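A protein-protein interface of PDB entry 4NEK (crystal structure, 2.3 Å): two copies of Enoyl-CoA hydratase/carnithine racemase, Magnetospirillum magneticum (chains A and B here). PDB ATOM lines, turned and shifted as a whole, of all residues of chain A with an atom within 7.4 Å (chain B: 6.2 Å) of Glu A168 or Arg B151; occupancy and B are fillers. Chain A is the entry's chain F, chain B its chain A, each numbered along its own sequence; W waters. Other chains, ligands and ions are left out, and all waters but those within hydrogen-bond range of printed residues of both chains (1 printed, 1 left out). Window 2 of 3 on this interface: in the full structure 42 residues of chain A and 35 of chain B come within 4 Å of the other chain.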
ATOM      1  N   ASP A 114      16.018 -25.701   1.063  1.00  0.00           N
ATOM      2  CA  ASP A 114      16.457 -24.501   0.356  1.00  0.00           C
ATOM      3  C   ASP A 114      15.264 -23.642  -0.107  1.00  0.00           C
ATOM      4  O   ASP A 114      15.331 -22.435  -0.049  1.00  0.00           O
ATOM      5  CB  ASP A 114      17.326 -24.893  -0.804  1.00  0.00           C
ATOM      6  CG  ASP A 114      18.540 -25.662  -0.352  1.00  0.00           C
ATOM      7  OD1 ASP A 114      19.443 -25.041   0.262  1.00  0.00           O
ATOM      8  OD2 ASP A 114      18.580 -26.904  -0.539  1.00  0.00           O
ATOM      9  N   LEU A 115      14.177 -24.275  -0.535  1.00  0.00           N
ATOM     10  CA  LEU A 115      12.939 -23.610  -0.790  1.00  0.00           C
ATOM     11  C   LEU A 115      11.781 -24.409  -0.223  1.00  0.00           C
ATOM     12  O   LEU A 115      11.770 -25.611  -0.319  1.00  0.00           O
ATOM     13  CB  LEU A 115      12.731 -23.502  -2.279  1.00  0.00           C
ATOM     14  CG  LEU A 115      13.769 -22.742  -3.068  1.00  0.00           C
ATOM     15  CD1 LEU A 115      13.458 -22.877  -4.531  1.00  0.00           C
ATOM     16  CD2 LEU A 115      13.764 -21.264  -2.718  1.00  0.00           C
ATOM     17  N   VAL A 116      10.754 -23.730   0.248  1.00  0.00           N
ATOM     18  CA  VAL A 116       9.575 -24.343   0.833  1.00  0.00           C
ATOM     19  C   VAL A 116       8.346 -23.561   0.455  1.00  0.00           C
ATOM     20  O   VAL A 116       8.287 -22.359   0.671  1.00  0.00           O
ATOM     21  CB  VAL A 116       9.675 -24.331   2.364  1.00  0.00           C
ATOM     22  CG1 VAL A 116       8.489 -25.015   2.980  1.00  0.00           C
ATOM     23  CG2 VAL A 116      10.939 -25.023   2.825  1.00  0.00           C
ATOM     24  N   TYR A 117       7.337 -24.234  -0.077  1.00  0.00           N
ATOM     25  CA  TYR A 117       6.030 -23.636  -0.334  1.00  0.00           C
ATOM     26  C   TYR A 117       5.001 -24.360   0.500  1.00  0.00           C
ATOM     27  O   TYR A 117       5.125 -25.538   0.722  1.00  0.00           O
ATOM     28  CB  TYR A 117       5.675 -23.759  -1.809  1.00  0.00           C
ATOM     29  CG  TYR A 117       6.731 -23.119  -2.614  1.00  0.00           C
ATOM     30  CD1 TYR A 117       6.685 -21.760  -2.901  1.00  0.00           C
ATOM     31  CD2 TYR A 117       7.838 -23.834  -3.020  1.00  0.00           C
ATOM     32  CE1 TYR A 117       7.701 -21.145  -3.633  1.00  0.00           C
ATOM     33  CE2 TYR A 117       8.870 -23.219  -3.731  1.00  0.00           C
ATOM     34  CZ  TYR A 117       8.796 -21.872  -4.033  1.00  0.00           C
ATOM     35  OH  TYR A 117       9.848 -21.300  -4.715  1.00  0.00           O
ATOM     36  N   PHE A 124       1.688 -25.404  11.579  1.00  0.00           N
ATOM     37  CA  PHE A 124       3.025 -25.733  11.989  1.00  0.00           C
ATOM     38  C   PHE A 124       3.012 -25.894  13.502  1.00  0.00           C
ATOM     39  O   PHE A 124       2.320 -25.145  14.191  1.00  0.00           O
ATOM     40  CB  PHE A 124       3.987 -24.635  11.611  1.00  0.00           C
ATOM     41  CG  PHE A 124       4.036 -24.353  10.167  1.00  0.00           C
ATOM     42  CD1 PHE A 124       3.130 -23.464   9.588  1.00  0.00           C
ATOM     43  CD2 PHE A 124       4.962 -24.962   9.362  1.00  0.00           C
ATOM     44  CE1 PHE A 124       3.180 -23.186   8.251  1.00  0.00           C
ATOM     45  CE2 PHE A 124       5.006 -24.703   7.991  1.00  0.00           C
ATOM     46  CZ  PHE A 124       4.143 -23.793   7.451  1.00  0.00           C
ATOM     47  N   ARG A 151       9.734 -14.768  19.429  1.00  0.00           N
ATOM     48  CA  ARG A 151       8.721 -15.459  18.655  1.00  0.00           C
ATOM     49  C   ARG A 151       9.016 -16.923  18.726  1.00  0.00           C
ATOM     50  O   ARG A 151       8.097 -17.701  18.657  1.00  0.00           O
ATOM     51  CB  ARG A 151       8.691 -15.138  17.153  1.00  0.00           C
ATOM     52  CG  ARG A 151       8.530 -13.670  16.863  1.00  0.00           C
ATOM     53  CD  ARG A 151       9.022 -12.955  15.589  1.00  0.00           C
ATOM     54  NE  ARG A 151       8.001 -12.646  14.597  1.00  0.00           N
ATOM     55  CZ  ARG A 151       8.258 -11.851  13.573  1.00  0.00           C
ATOM     56  NH1 ARG A 151       9.511 -11.404  13.397  1.00  0.00           N
ATOM     57  NH2 ARG A 151       7.297 -11.542  12.719  1.00  0.00           N
ATOM     58  N   PHE A 162       1.438 -22.533  14.975  1.00  0.00           N
ATOM     59  CA  PHE A 162       1.365 -21.269  14.273  1.00  0.00           C
ATOM     60  C   PHE A 162       1.086 -21.576  12.832  1.00  0.00           C
ATOM     61  O   PHE A 162       1.090 -22.750  12.424  1.00  0.00           O
ATOM     62  CB  PHE A 162       2.640 -20.475  14.438  1.00  0.00           C
ATOM     63  CG  PHE A 162       3.880 -21.173  13.933  1.00  0.00           C
ATOM     64  CD1 PHE A 162       4.574 -22.041  14.750  1.00  0.00           C
ATOM     65  CD2 PHE A 162       4.364 -20.921  12.636  1.00  0.00           C
ATOM     66  CE1 PHE A 162       5.716 -22.682  14.298  1.00  0.00           C
ATOM     67  CE2 PHE A 162       5.536 -21.498  12.208  1.00  0.00           C
ATOM     68  CZ  PHE A 162       6.207 -22.398  13.031  1.00  0.00           C
ATOM     69  N   GLY A 163       0.809 -20.519  12.086  1.00  0.00           N
ATOM     70  CA  GLY A 163       0.268 -20.615  10.738  1.00  0.00           C
ATOM     71  C   GLY A 163       1.175 -19.973   9.728  1.00  0.00           C
ATOM     72  O   GLY A 163       2.302 -19.592  10.023  1.00  0.00           O
ATOM     73  N   VAL A 164       0.668 -19.889   8.520  1.00  0.00           N
ATOM     74  CA  VAL A 164       1.446 -19.433   7.357  1.00  0.00           C
ATOM     75  C   VAL A 164       1.835 -17.973   7.446  1.00  0.00           C
ATOM     76  O   VAL A 164       2.859 -17.574   6.881  1.00  0.00           O
ATOM     77  CB  VAL A 164       0.691 -19.688   6.030  1.00  0.00           C
ATOM     78  CG1 VAL A 164       0.567 -21.167   5.793  1.00  0.00           C
ATOM     79  CG2 VAL A 164      -0.693 -19.058   6.027  1.00  0.00           C
ATOM     80  N   ASP A 165       1.032 -17.182   8.141  1.00  0.00           N
ATOM     81  CA  ASP A 165       1.419 -15.840   8.379  1.00  0.00           C
ATOM     82  C   ASP A 165       2.812 -15.787   9.049  1.00  0.00           C
ATOM     83  O   ASP A 165       3.718 -15.086   8.588  1.00  0.00           O
ATOM     84  CB  ASP A 165       0.363 -15.094   9.215  1.00  0.00           C
ATOM     85  CG  ASP A 165       0.021 -15.784  10.566  1.00  0.00           C
ATOM     86  OD1 ASP A 165       0.232 -17.007  10.782  1.00  0.00           O
ATOM     87  OD2 ASP A 165      -0.520 -15.067  11.440  1.00  0.00           O
ATOM     88  N   THR A 166       2.959 -16.462  10.168  1.00  0.00           N
ATOM     89  CA  THR A 166       4.171 -16.390  10.912  1.00  0.00           C
ATOM     90  C   THR A 166       5.247 -17.062  10.116  1.00  0.00           C
ATOM     91  O   THR A 166       6.383 -16.593  10.066  1.00  0.00           O
ATOM     92  CB  THR A 166       3.984 -17.080  12.260  1.00  0.00           C
ATOM     93  OG1 THR A 166       2.936 -16.406  12.971  1.00  0.00           O
ATOM     94  CG2 THR A 166       5.254 -17.063  13.092  1.00  0.00           C
ATOM     95  N   ALA A 167       4.904 -18.172   9.488  1.00  0.00           N
ATOM     96  CA  ALA A 167       5.927 -18.983   8.840  1.00  0.00           C
ATOM     97  C   ALA A 167       6.580 -18.200   7.709  1.00  0.00           C
ATOM     98  O   ALA A 167       7.800 -18.232   7.556  1.00  0.00           O
ATOM     99  CB  ALA A 167       5.334 -20.246   8.296  1.00  0.00           C
ATOM    100  N   GLU A 168       5.788 -17.457   6.959  1.00  0.00           N
ATOM    101  CA  GLU A 168       6.366 -16.617   5.950  1.00  0.00           C
ATOM    102  C   GLU A 168       7.085 -15.444   6.572  1.00  0.00           C
ATOM    103  O   GLU A 168       8.164 -15.086   6.145  1.00  0.00           O
ATOM    104  CB  GLU A 168       5.346 -16.146   4.921  1.00  0.00           C
ATOM    105  CG  GLU A 168       6.033 -15.401   3.796  1.00  0.00           C
ATOM    106  CD  GLU A 168       5.180 -15.202   2.519  1.00  0.00           C
ATOM    107  OE1 GLU A 168       3.994 -15.580   2.511  1.00  0.00           O
ATOM    108  OE2 GLU A 168       5.706 -14.660   1.493  1.00  0.00           O
ATOM    109  N   ALA A 169       6.528 -14.848   7.605  1.00  0.00           N
ATOM    110  CA  ALA A 169       7.163 -13.670   8.166  1.00  0.00           C
ATOM    111  C   ALA A 169       8.551 -13.993   8.707  1.00  0.00           C
ATOM    112  O   ALA A 169       9.445 -13.207   8.545  1.00  0.00           O
ATOM    113  CB  ALA A 169       6.305 -13.063   9.263  1.00  0.00           C
ATOM    114  N   VAL A 170       8.755 -15.130   9.338  1.00  0.00           N
ATOM    115  CA  VAL A 170      10.069 -15.406   9.858  1.00  0.00           C
ATOM    116  C   VAL A 170      10.990 -16.132   8.864  1.00  0.00           C
ATOM    117  O   VAL A 170      12.092 -16.528   9.240  1.00  0.00           O
ATOM    118  CB  VAL A 170       9.999 -16.208  11.163  1.00  0.00           C
ATOM    119  CG1 VAL A 170       9.055 -15.525  12.123  1.00  0.00           C
ATOM    120  CG2 VAL A 170       9.536 -17.638  10.925  1.00  0.00           C
ATOM    121  N   GLY A 171      10.545 -16.347   7.635  1.00  0.00           N
ATOM    122  CA  GLY A 171      11.414 -16.958   6.629  1.00  0.00           C
ATOM    123  C   GLY A 171      11.524 -18.483   6.677  1.00  0.00           C
ATOM    124  O   GLY A 171      12.488 -19.087   6.160  1.00  0.00           O
ATOM    125  N   LEU A 172      10.538 -19.118   7.305  1.00  0.00           N
ATOM    126  CA  LEU A 172      10.475 -20.546   7.325  1.00  0.00           C
ATOM    127  C   LEU A 172       9.971 -21.083   5.980  1.00  0.00           C
ATOM    128  O   LEU A 172      10.365 -22.168   5.596  1.00  0.00           O
ATOM    129  CB  LEU A 172       9.547 -21.000   8.412  1.00  0.00           C
ATOM    130  CG  LEU A 172       9.607 -22.477   8.735  1.00  0.00           C
ATOM    131  CD1 LEU A 172      10.968 -22.929   9.296  1.00  0.00           C
ATOM    132  CD2 LEU A 172       8.529 -22.785   9.745  1.00  0.00           C
ATOM    133  N   ILE A 173       9.137 -20.311   5.269  1.00  0.00           N
ATOM    134  CA  ILE A 173       8.681 -20.702   3.960  1.00  0.00           C
ATOM    135  C   ILE A 173       8.813 -19.542   3.021  1.00  0.00           C
ATOM    136  O   ILE A 173       8.881 -18.412   3.453  1.00  0.00           O
ATOM    137  CB  ILE A 173       7.201 -21.109   3.943  1.00  0.00           C
ATOM    138  CG1 ILE A 173       6.312 -19.933   4.323  1.00  0.00           C
ATOM    139  CG2 ILE A 173       6.964 -22.256   4.887  1.00  0.00           C
ATOM    140  CD1 ILE A 173       4.852 -20.297   4.393  1.00  0.00           C
ATOM    141  N   ASN A 174       8.822 -19.831   1.728  1.00  0.00           N
ATOM    142  CA  ASN A 174       8.967 -18.799   0.725  1.00  0.00           C
ATOM    143  C   ASN A 174       7.621 -18.182   0.423  1.00  0.00           C
ATOM    144  O   ASN A 174       7.558 -17.041   0.009  1.00  0.00           O
ATOM    145  CB  ASN A 174       9.538 -19.357  -0.578  1.00  0.00           C
ATOM    146  CG  ASN A 174      11.013 -19.706  -0.477  1.00  0.00           C
ATOM    147  OD1 ASN A 174      11.890 -18.932  -0.858  1.00  0.00           O
ATOM    148  ND2 ASN A 174      11.286 -20.837   0.054  1.00  0.00           N
ATOM    149  N   GLY A 175       6.544 -18.935   0.582  1.00  0.00           N
ATOM    150  CA  GLY A 175       5.275 -18.442   0.126  1.00  0.00           C
ATOM    151  C   GLY A 175       4.157 -19.403   0.242  1.00  0.00           C
ATOM    152  O   GLY A 175       4.367 -20.589   0.479  1.00  0.00           O
ATOM    153  N   VAL A 176       2.943 -18.880   0.053  1.00  0.00           N
ATOM    154  CA  VAL A 176       1.728 -19.655   0.206  1.00  0.00           C
ATOM    155  C   VAL A 176       1.105 -19.875  -1.137  1.00  0.00           C
ATOM    156  O   VAL A 176       1.031 -18.967  -1.904  1.00  0.00           O
ATOM    157  CB  VAL A 176       0.771 -18.911   1.084  1.00  0.00           C
ATOM    158  CG1 VAL A 176      -0.518 -19.667   1.240  1.00  0.00           C
ATOM    159  CG2 VAL A 176       1.400 -18.742   2.459  1.00  0.00           C
ATOM    160  N   MET A 208      26.553 -20.770   1.411  1.00  0.00           N
ATOM    161  CA  MET A 208      25.426 -20.217   2.166  1.00  0.00           C
ATOM    162  C   MET A 208      25.276 -20.901   3.493  1.00  0.00           C
ATOM    163  O   MET A 208      24.951 -20.253   4.477  1.00  0.00           O
ATOM    164  CB  MET A 208      24.099 -20.397   1.478  1.00  0.00           C
ATOM    165  CG  MET A 208      24.005 -19.375   0.370  1.00  0.00           C
ATOM    166  SD  MET A 208      22.398 -19.764  -0.690  1.00  0.00           S
ATOM    167  CE  MET A 208      21.007 -19.110   0.545  1.00  0.00           C
ATOM    168  N   ALA B 147      17.815 -12.464   5.460  1.00  0.00           N
ATOM    169  CA  ALA B 147      16.550 -12.891   4.891  1.00  0.00           C
ATOM    170  C   ALA B 147      16.123 -14.262   5.367  1.00  0.00           C
ATOM    171  O   ALA B 147      14.998 -14.713   5.065  1.00  0.00           O
ATOM    172  CB  ALA B 147      16.684 -12.890   3.397  1.00  0.00           C
ATOM    173  N   GLY B 148      17.035 -14.977   6.024  1.00  0.00           N
ATOM    174  CA  GLY B 148      16.867 -16.393   6.210  1.00  0.00           C
ATOM    175  C   GLY B 148      17.271 -17.167   4.975  1.00  0.00           C
ATOM    176  O   GLY B 148      17.261 -16.654   3.827  1.00  0.00           O
ATOM    177  N   HIS B 149      17.571 -18.450   5.174  1.00  0.00           N
ATOM    178  CA  HIS B 149      18.131 -19.230   4.095  1.00  0.00           C
ATOM    179  C   HIS B 149      17.206 -19.339   2.869  1.00  0.00           C
ATOM    180  O   HIS B 149      17.684 -19.335   1.714  1.00  0.00           O
ATOM    181  CB  HIS B 149      18.499 -20.608   4.601  1.00  0.00           C
ATOM    182  CG  HIS B 149      19.128 -21.447   3.553  1.00  0.00           C
ATOM    183  ND1 HIS B 149      20.439 -21.292   3.174  1.00  0.00           N
ATOM    184  CD2 HIS B 149      18.607 -22.398   2.738  1.00  0.00           C
ATOM    185  CE1 HIS B 149      20.714 -22.133   2.187  1.00  0.00           C
ATOM    186  NE2 HIS B 149      19.613 -22.802   1.890  1.00  0.00           N
ATOM    187  N   ARG B 150      15.894 -19.471   3.095  1.00  0.00           N
ATOM    188  CA  ARG B 150      15.027 -19.742   1.967  1.00  0.00           C
ATOM    189  C   ARG B 150      14.806 -18.564   1.070  1.00  0.00           C
ATOM    190  O   ARG B 150      14.751 -18.709  -0.140  1.00  0.00           O
ATOM    191  CB  ARG B 150      13.709 -20.332   2.432  1.00  0.00           C
ATOM    192  CG  ARG B 150      13.884 -21.845   2.641  1.00  0.00           C
ATOM    193  CD  ARG B 150      13.175 -22.354   3.859  1.00  0.00           C
ATOM    194  NE  ARG B 150      13.573 -21.645   5.054  1.00  0.00           N
ATOM    195  CZ  ARG B 150      14.707 -21.858   5.704  1.00  0.00           C
ATOM    196  NH1 ARG B 150      15.575 -22.788   5.309  1.00  0.00           N
ATOM    197  NH2 ARG B 150      14.960 -21.148   6.768  1.00  0.00           N
ATOM    198  N   ARG B 151      14.664 -17.394   1.660  1.00  0.00           N
ATOM    199  CA  ARG B 151      14.403 -16.225   0.855  1.00  0.00           C
ATOM    200  C   ARG B 151      15.721 -15.845   0.193  1.00  0.00           C
ATOM    201  O   ARG B 151      15.717 -15.436  -0.961  1.00  0.00           O
ATOM    202  CB  ARG B 151      13.728 -15.113   1.685  1.00  0.00           C
ATOM    203  CG  ARG B 151      13.480 -13.850   0.884  1.00  0.00           C
ATOM    204  CD  ARG B 151      12.268 -13.938  -0.030  1.00  0.00           C
ATOM    205  NE  ARG B 151      11.030 -13.906   0.777  1.00  0.00           N
ATOM    206  CZ  ARG B 151       9.876 -14.529   0.477  1.00  0.00           C
ATOM    207  NH1 ARG B 151       9.739 -15.253  -0.645  1.00  0.00           N
ATOM    208  NH2 ARG B 151       8.840 -14.447   1.321  1.00  0.00           N
ATOM    209  N   ALA B 152      16.845 -16.056   0.874  1.00  0.00           N
ATOM    210  CA  ALA B 152      18.145 -15.858   0.241  1.00  0.00           C
ATOM    211  C   ALA B 152      18.400 -16.829  -0.893  1.00  0.00           C
ATOM    212  O   ALA B 152      19.093 -16.504  -1.826  1.00  0.00           O
ATOM    213  CB  ALA B 152      19.271 -15.982   1.260  1.00  0.00           C
ATOM    214  N   ALA B 153      17.873 -18.041  -0.806  1.00  0.00           N
ATOM    215  CA  ALA B 153      18.013 -18.982  -1.915  1.00  0.00           C
ATOM    216  C   ALA B 153      17.290 -18.509  -3.167  1.00  0.00           C
ATOM    217  O   ALA B 153      17.751 -18.806  -4.255  1.00  0.00           O
ATOM    218  CB  ALA B 153      17.509 -20.356  -1.534  1.00  0.00           C
ATOM    219  N   GLU B 154      16.168 -17.794  -3.044  1.00  0.00           N
ATOM    220  CA  GLU B 154      15.564 -17.182  -4.253  1.00  0.00           C
ATOM    221  C   GLU B 154      16.564 -16.257  -4.938  1.00  0.00           C
ATOM    222  O   GLU B 154      16.609 -16.158  -6.160  1.00  0.00           O
ATOM    223  CB  GLU B 154      14.313 -16.367  -3.935  1.00  0.00           C
ATOM    224  CG  GLU B 154      13.100 -17.163  -3.567  1.00  0.00           C
ATOM    225  CD  GLU B 154      11.886 -16.289  -3.202  1.00  0.00           C
ATOM    226  OE1 GLU B 154      11.550 -15.335  -3.951  1.00  0.00           O
ATOM    227  OE2 GLU B 154      11.170 -16.628  -2.240  1.00  0.00           O
ATOM    228  N   MET B 155      17.332 -15.542  -4.135  1.00  0.00           N
ATOM    229  CA  MET B 155      18.218 -14.550  -4.669  1.00  0.00           C
ATOM    230  C   MET B 155      19.456 -15.164  -5.251  1.00  0.00           C
ATOM    231  O   MET B 155      19.868 -14.813  -6.356  1.00  0.00           O
ATOM    232  CB  MET B 155      18.675 -13.576  -3.565  1.00  0.00           C
ATOM    233  CG  MET B 155      17.531 -12.850  -2.876  1.00  0.00           C
ATOM    234  SD  MET B 155      18.042 -11.923  -1.183  1.00  0.00           S
ATOM    235  CE  MET B 155      19.807 -11.298  -1.753  1.00  0.00           C
ATOM    236  N   LEU B 156      20.059 -16.084  -4.511  1.00  0.00           N
ATOM    237  CA  LEU B 156      21.360 -16.618  -4.861  1.00  0.00           C
ATOM    238  C   LEU B 156      21.354 -17.955  -5.635  1.00  0.00           C
ATOM    239  O   LEU B 156      22.242 -18.201  -6.445  1.00  0.00           O
ATOM    240  CB  LEU B 156      22.176 -16.817  -3.603  1.00  0.00           C
ATOM    241  CG  LEU B 156      22.376 -15.573  -2.770  1.00  0.00           C
ATOM    242  CD1 LEU B 156      23.253 -15.851  -1.578  1.00  0.00           C
ATOM    243  CD2 LEU B 156      22.993 -14.474  -3.612  1.00  0.00           C
ATOM    244  N   THR B 166      10.776  -6.749  -0.856  1.00  0.00           N
ATOM    245  CA  THR B 166      11.601  -7.709  -0.241  1.00  0.00           C
ATOM    246  C   THR B 166      12.773  -7.020   0.434  1.00  0.00           C
ATOM    247  O   THR B 166      13.143  -7.366   1.548  1.00  0.00           O
ATOM    248  CB  THR B 166      12.080  -8.710  -1.293  1.00  0.00           C
ATOM    249  OG1 THR B 166      10.938  -9.313  -1.894  1.00  0.00           O
ATOM    250  CG2 THR B 166      12.952  -9.809  -0.675  1.00  0.00           C
ATOM    251  N   VAL B 170      13.510  -7.685   4.396  1.00  0.00           N
ATOM    252  CA  VAL B 170      14.642  -8.381   4.973  1.00  0.00           C
ATOM    253  C   VAL B 170      15.726  -7.479   5.538  1.00  0.00           C
ATOM    254  O   VAL B 170      16.768  -7.982   5.984  1.00  0.00           O
ATOM    255  CB  VAL B 170      15.288  -9.336   3.969  1.00  0.00           C
ATOM    256  CG1 VAL B 170      14.230 -10.230   3.364  1.00  0.00           C
ATOM    257  CG2 VAL B 170      16.048  -8.606   2.880  1.00  0.00           C
HETATM  258  O   HOH W   1      22.217 -20.517   5.101  1.00  0.00           O
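Hydrophobic or aromatic side chains of chain A within 4 Å of the printed part of chain B: Leu A115, Val A116 and Met A208.
Among the printed residues, Asp or Glu carboxylates within 4 Å of a Lys or Arg side-chain nitrogen of the other chain: Glu A168 with Arg B151 (3.1 Å).
Water W1 lies within hydrogen-bond range of a ring nitrogen (ND1) of His B149 (2.7 Å) and the backbone carbonyl oxygen (O) of Met A208 (2.8 Å).
Arg B150 touches Asp A114 (CG to O, 3.1 Å).
CB of Ala B153 touches O of Asp A114 (3.4 Å).
O of Arg B150 touches CD2 of Leu A115, at 3.8 Å.
CG2 of Val A116 touches CD of Arg B150 (3.6 Å).
Met A208 touches His B149.
CE of Met A208 touches CB of Ala B152 (3.6 Å).
Met A208 touches Ala B153 (CE to N, 3.6 Å).
Printed residues of chain B within 4 Å of Val A116: Arg B150 (3.6 Å).
Glu A168 touches just one residue of chain B: Arg B151 (3.1 Å).
Ala A169 touches none of the printed residues of chain B.
Of the printed residues of chain B, Asn A174 touches Arg B150 (3.0 Å), Arg B151 (2.9 Å) and Glu B154 (2.8 Å).
Ala B147 touches none of the printed residues of chain A.
Of the printed residues of chain A, Arg B150 touches Asp A114 (3.1 Å), Leu A115 (3.8 Å), Val A116 (3.6 Å), Gly A171 (3.0 Å), Leu A172 (3.3 Å) and Asn A174 (3.0 Å).
The nearest printed residue of chain B that does not touch Glu A168 is Glu B154 (6.9 Å).
The nearest residue of chain A that does not touch Arg B151 is Ile A173 (4.5 Å).
3 positions are printed for both chains.
Of the 14 pairs that touch across the chains among the printed residues, none has its exchanged pair printed and touching as well.
The backbone carbonyl oxygen of Ala A167 lies within hydrogen-bond range of the backbone NH of Leu A172 (2.9 Å).
The backbone carbonyl oxygen (O) of Val A116 lies within hydrogen-bond range of the backbone NH (N) of Asn A174 (2.8 Å).
OE2 of Glu B154 is in salt-bridge range of NH1 of Arg B151 (2.5 Å).
The guanidinium group (NH1) of Arg B151 lies within hydrogen-bond range of the backbone carbonyl oxygen (O) of Asn A174 (2.9 Å).
The backbone carbonyl oxygen (O) of Leu A172 is in hydrogen-bond range of the guanidinium group (NE) of Arg B150.
The side-chain amide oxygen of Asn A174 sits close to the side-chain carboxylate of Glu B154.
A ring nitrogen (NE2) of His B149 is in hydrogen-bond range of the side-chain carboxylate (OD1) of Asp A114.
The backbone carbonyl oxygen of Arg B150 lies close to the side-chain amide oxygen of Asn A174 (3.0 Å).
The backbone carbonyl oxygen (O) of Gly A171 sits at hydrogen-bond distance from the guanidinium group (NE) of Arg B150, 3.0 Å away.
The side-chain carboxylate (OE2) of Glu A168 lies within salt-bridge range of the guanidinium group (NH2) of Arg B151 (3.1 Å).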
